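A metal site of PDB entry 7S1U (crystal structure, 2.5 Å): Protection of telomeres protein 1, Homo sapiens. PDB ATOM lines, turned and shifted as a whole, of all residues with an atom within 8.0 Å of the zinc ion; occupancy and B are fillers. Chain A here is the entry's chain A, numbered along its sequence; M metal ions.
The backbone carbonyl oxygen (O) of Val 206 sits at hydrogen-bond distance from the backbone NH (N) of Cys 173. SG of Cys 55 lies close to N of Leu 57 (3.4 Å). The backbone carbonyl oxygen of Cys 173 is in hydrogen-bond range of the side-chain hydroxyl of Ser 177 (2.7 Å). The backbone NH (N) of Cys 52 sits at hydrogen-bond distance from the backbone carbonyl oxygen (O) of Leu 57 (3.0 Å). SG of Cys 52 lies close to N of Lys 54 (3.4 Å).
Within 4 Å of the zinc ion: Cys 52, Cys 55, Cys 173 and Cys 176.
The side-chain sulfur (SG) of Cys 52 binds the zinc ion (2.3 Å). The zinc ion is bound by the side-chain sulfur (SG) of Cys 176, at 2.3 Å. The zinc ion is bound by SG of Cys 173, at 2.3 Å. The side-chain sulfur (SG) of Cys 55 binds the zinc ion, at 2.3 Å. The zinc ion has four donor atoms within binding distance.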
ATOM      1  N   HIS A  51      -9.653 -12.275  10.560  1.00  0.00           N
ATOM      2  CA  HIS A  51      -9.521 -12.563  11.992  1.00  0.00           C
ATOM      3  C   HIS A  51      -8.253 -13.351  12.237  1.00  0.00           C
ATOM      4  O   HIS A  51      -8.037 -14.375  11.589  1.00  0.00           O
ATOM      5  CB  HIS A  51     -10.733 -13.338  12.488  1.00  0.00           C
ATOM      6  CG  HIS A  51     -10.504 -14.094  13.753  1.00  0.00           C
ATOM      7  ND1 HIS A  51     -10.319 -15.458  13.753  1.00  0.00           N
ATOM      8  CD2 HIS A  51     -10.490 -13.703  15.050  1.00  0.00           C
ATOM      9  CE1 HIS A  51     -10.150 -15.863  15.003  1.00  0.00           C
ATOM     10  NE2 HIS A  51     -10.249 -14.818  15.803  1.00  0.00           N
ATOM     11  N   CYS A  52      -7.422 -12.891  13.160  1.00  0.00           N
ATOM     12  CA  CYS A  52      -6.250 -13.660  13.550  1.00  0.00           C
ATOM     13  C   CYS A  52      -6.683 -14.820  14.430  1.00  0.00           C
ATOM     14  O   CYS A  52      -7.424 -14.609  15.400  1.00  0.00           O
ATOM     15  CB  CYS A  52      -5.252 -12.790  14.295  1.00  0.00           C
ATOM     16  SG  CYS A  52      -3.819 -13.740  14.871  1.00  0.00           S
ATOM     17  N   PRO A  53      -6.247 -16.045  14.132  1.00  0.00           N
ATOM     18  CA  PRO A  53      -6.647 -17.177  14.970  1.00  0.00           C
ATOM     19  C   PRO A  53      -6.003 -17.163  16.348  1.00  0.00           C
ATOM     20  O   PRO A  53      -6.546 -17.780  17.263  1.00  0.00           O
ATOM     21  CB  PRO A  53      -6.177 -18.391  14.157  1.00  0.00           C
ATOM     22  CG  PRO A  53      -5.060 -17.876  13.317  1.00  0.00           C
ATOM     23  CD  PRO A  53      -5.368 -16.437  13.026  1.00  0.00           C
ATOM     24  N   LYS A  54      -4.888 -16.462  16.520  1.00  0.00           N
ATOM     25  CA  LYS A  54      -4.163 -16.441  17.783  1.00  0.00           C
ATOM     26  C   LYS A  54      -4.524 -15.237  18.653  1.00  0.00           C
ATOM     27  O   LYS A  54      -4.836 -15.398  19.831  1.00  0.00           O
ATOM     28  CB  LYS A  54      -2.648 -16.462  17.514  1.00  0.00           C
ATOM     29  CG  LYS A  54      -1.804 -15.952  18.672  1.00  0.00           C
ATOM     30  CD  LYS A  54      -0.360 -15.768  18.249  1.00  0.00           C
ATOM     31  CE  LYS A  54       0.567 -15.717  19.447  1.00  0.00           C
ATOM     32  NZ  LYS A  54       1.957 -15.364  19.055  1.00  0.00           N
ATOM     33  N   CYS A  55      -4.479 -14.032  18.089  1.00  0.00           N
ATOM     34  CA  CYS A  55      -4.768 -12.825  18.839  1.00  0.00           C
ATOM     35  C   CYS A  55      -6.228 -12.410  18.765  1.00  0.00           C
ATOM     36  O   CYS A  55      -6.644 -11.513  19.509  1.00  0.00           O
ATOM     37  CB  CYS A  55      -3.887 -11.667  18.356  1.00  0.00           C
ATOM     38  SG  CYS A  55      -4.627 -10.732  17.015  1.00  0.00           S
ATOM     39  N   HIS A  56      -7.012 -13.017  17.875  1.00  0.00           N
ATOM     40  CA  HIS A  56      -8.468 -12.856  17.798  1.00  0.00           C
ATOM     41  C   HIS A  56      -8.889 -11.446  17.400  1.00  0.00           C
ATOM     42  O   HIS A  56     -10.026 -11.045  17.692  1.00  0.00           O
ATOM     43  CB  HIS A  56      -9.141 -13.246  19.120  1.00  0.00           C
ATOM     44  CG  HIS A  56      -9.096 -14.715  19.407  1.00  0.00           C
ATOM     45  ND1 HIS A  56      -9.477 -15.663  18.497  1.00  0.00           N
ATOM     46  CD2 HIS A  56      -8.702 -15.382  20.515  1.00  0.00           C
ATOM     47  CE1 HIS A  56      -9.333 -16.870  19.026  1.00  0.00           C
ATOM     48  NE2 HIS A  56      -8.874 -16.725  20.254  1.00  0.00           N
ATOM     49  N   LEU A  57      -8.032 -10.680  16.734  1.00  0.00           N
ATOM     50  CA  LEU A  57      -8.445  -9.377  16.245  1.00  0.00           C
ATOM     51  C   LEU A  57      -9.124  -9.508  14.894  1.00  0.00           C
ATOM     52  O   LEU A  57      -8.708 -10.303  14.041  1.00  0.00           O
ATOM     53  CB  LEU A  57      -7.256  -8.411  16.145  1.00  0.00           C
ATOM     54  CG  LEU A  57      -6.281  -8.348  14.960  1.00  0.00           C
ATOM     55  CD1 LEU A  57      -6.838  -7.534  13.788  1.00  0.00           C
ATOM     56  CD2 LEU A  57      -4.966  -7.742  15.407  1.00  0.00           C
ATOM     57  N   LEU A  58     -10.191  -8.742  14.698  1.00  0.00           N
ATOM     58  CA  LEU A  58     -10.922  -8.677  13.445  1.00  0.00           C
ATOM     59  C   LEU A  58     -10.663  -7.329  12.789  1.00  0.00           C
ATOM     60  O   LEU A  58     -10.728  -6.292  13.461  1.00  0.00           O
ATOM     61  CB  LEU A  58     -12.419  -8.879  13.682  1.00  0.00           C
ATOM     62  CG  LEU A  58     -13.288  -9.287  12.487  1.00  0.00           C
ATOM     63  CD1 LEU A  58     -13.020 -10.722  12.083  1.00  0.00           C
ATOM     64  CD2 LEU A  58     -14.760  -9.110  12.822  1.00  0.00           C
ATOM     65  N   GLY A 172      -1.341 -12.314   6.687  1.00  0.00           N
ATOM     66  CA  GLY A 172      -0.871 -12.692   8.008  1.00  0.00           C
ATOM     67  C   GLY A 172      -1.165 -11.593   9.023  1.00  0.00           C
ATOM     68  O   GLY A 172      -1.555 -10.476   8.672  1.00  0.00           O
ATOM     69  N   CYS A 173      -0.971 -11.939  10.291  1.00  0.00           N
ATOM     70  CA  CYS A 173      -1.199 -10.974  11.360  1.00  0.00           C
ATOM     71  C   CYS A 173       0.025 -10.089  11.542  1.00  0.00           C
ATOM     72  O   CYS A 173       1.164 -10.571  11.521  1.00  0.00           O
ATOM     73  CB  CYS A 173      -1.520 -11.685  12.670  1.00  0.00           C
ATOM     74  SG  CYS A 173      -2.387 -10.623  13.842  1.00  0.00           S
ATOM     75  N   LYS A 174      -0.215  -8.793  11.727  1.00  0.00           N
ATOM     76  CA  LYS A 174       0.878  -7.826  11.740  1.00  0.00           C
ATOM     77  C   LYS A 174       1.778  -8.011  12.957  1.00  0.00           C
ATOM     78  O   LYS A 174       2.981  -8.257  12.825  1.00  0.00           O
ATOM     79  CB  LYS A 174       0.323  -6.409  11.687  1.00  0.00           C
ATOM     80  CG  LYS A 174       1.374  -5.336  11.506  1.00  0.00           C
ATOM     81  CD  LYS A 174       1.929  -5.362  10.087  1.00  0.00           C
ATOM     82  CE  LYS A 174       2.887  -4.213   9.859  1.00  0.00           C
ATOM     83  NZ  LYS A 174       2.188  -2.911   9.806  1.00  0.00           N
ATOM     84  N   GLN A 175       1.204  -7.901  14.156  1.00  0.00           N
ATOM     85  CA  GLN A 175       1.986  -7.988  15.376  1.00  0.00           C
ATOM     86  C   GLN A 175       2.189  -9.417  15.862  1.00  0.00           C
ATOM     87  O   GLN A 175       3.172  -9.694  16.552  1.00  0.00           O
ATOM     88  CB  GLN A 175       1.318  -7.162  16.480  1.00  0.00           C
ATOM     89  CG  GLN A 175       0.651  -5.886  15.992  1.00  0.00           C
ATOM     90  CD  GLN A 175       1.648  -4.850  15.528  1.00  0.00           C
ATOM     91  OE1 GLN A 175       2.789  -4.810  15.997  1.00  0.00           O
ATOM     92  NE2 GLN A 175       1.231  -3.991  14.607  1.00  0.00           N
ATOM     93  N   CYS A 176       1.286 -10.326  15.503  1.00  0.00           N
ATOM     94  CA  CYS A 176       1.434 -11.717  15.946  1.00  0.00           C
ATOM     95  C   CYS A 176       2.527 -12.421  15.155  1.00  0.00           C
ATOM     96  O   CYS A 176       3.270 -13.242  15.719  1.00  0.00           O
ATOM     97  CB  CYS A 176       0.108 -12.461  15.798  1.00  0.00           C
ATOM     98  SG  CYS A 176      -1.088 -12.118  17.091  1.00  0.00           S
ATOM     99  N   SER A 177       2.657 -12.129  13.868  1.00  0.00           N
ATOM    100  CA  SER A 177       3.663 -12.777  13.057  1.00  0.00           C
ATOM    101  C   SER A 177       5.028 -12.134  13.263  1.00  0.00           C
ATOM    102  O   SER A 177       5.145 -11.003  13.761  1.00  0.00           O
ATOM    103  CB  SER A 177       3.284 -12.725  11.578  1.00  0.00           C
ATOM    104  OG  SER A 177       1.941 -13.103  11.388  1.00  0.00           O
ATOM    105  N   VAL A 206       1.380 -15.732  11.050  1.00  0.00           N
ATOM    106  CA  VAL A 206       0.112 -16.223  11.577  1.00  0.00           C
ATOM    107  C   VAL A 206      -0.970 -15.920  10.543  1.00  0.00           C
ATOM    108  O   VAL A 206      -1.399 -14.764  10.420  1.00  0.00           O
ATOM    109  CB  VAL A 206      -0.213 -15.598  12.935  1.00  0.00           C
ATOM    110  CG1 VAL A 206      -1.388 -16.307  13.584  1.00  0.00           C
ATOM    111  CG2 VAL A 206       0.995 -15.628  13.846  1.00  0.00           C
ATOM    112  N   PRO A 207      -1.437 -16.911   9.787  1.00  0.00           N
ATOM    113  CA  PRO A 207      -2.362 -16.634   8.681  1.00  0.00           C
ATOM    114  C   PRO A 207      -3.750 -16.254   9.195  1.00  0.00           C
ATOM    115  O   PRO A 207      -4.313 -16.927  10.055  1.00  0.00           O
ATOM    116  CB  PRO A 207      -2.406 -17.955   7.900  1.00  0.00           C
ATOM    117  CG  PRO A 207      -1.274 -18.793   8.449  1.00  0.00           C
ATOM    118  CD  PRO A 207      -1.089 -18.340   9.854  1.00  0.00           C
ATOM    119  N   LEU A 208      -4.290 -15.165   8.645  1.00  0.00           N
ATOM    120  CA  LEU A 208      -5.665 -14.776   8.917  1.00  0.00           C
ATOM    121  C   LEU A 208      -6.608 -15.515   7.958  1.00  0.00           C
ATOM    122  O   LEU A 208      -6.261 -15.771   6.806  1.00  0.00           O
ATOM    123  CB  LEU A 208      -5.837 -13.263   8.767  1.00  0.00           C
ATOM    124  CG  LEU A 208      -4.677 -12.366   9.199  1.00  0.00           C
ATOM    125  CD1 LEU A 208      -4.975 -10.908   8.919  1.00  0.00           C
ATOM    126  CD2 LEU A 208      -4.362 -12.569  10.672  1.00  0.00           C
HETATM  127 ZN    ZN M   1      -2.963 -11.784  15.767  1.00  0.00          ZN
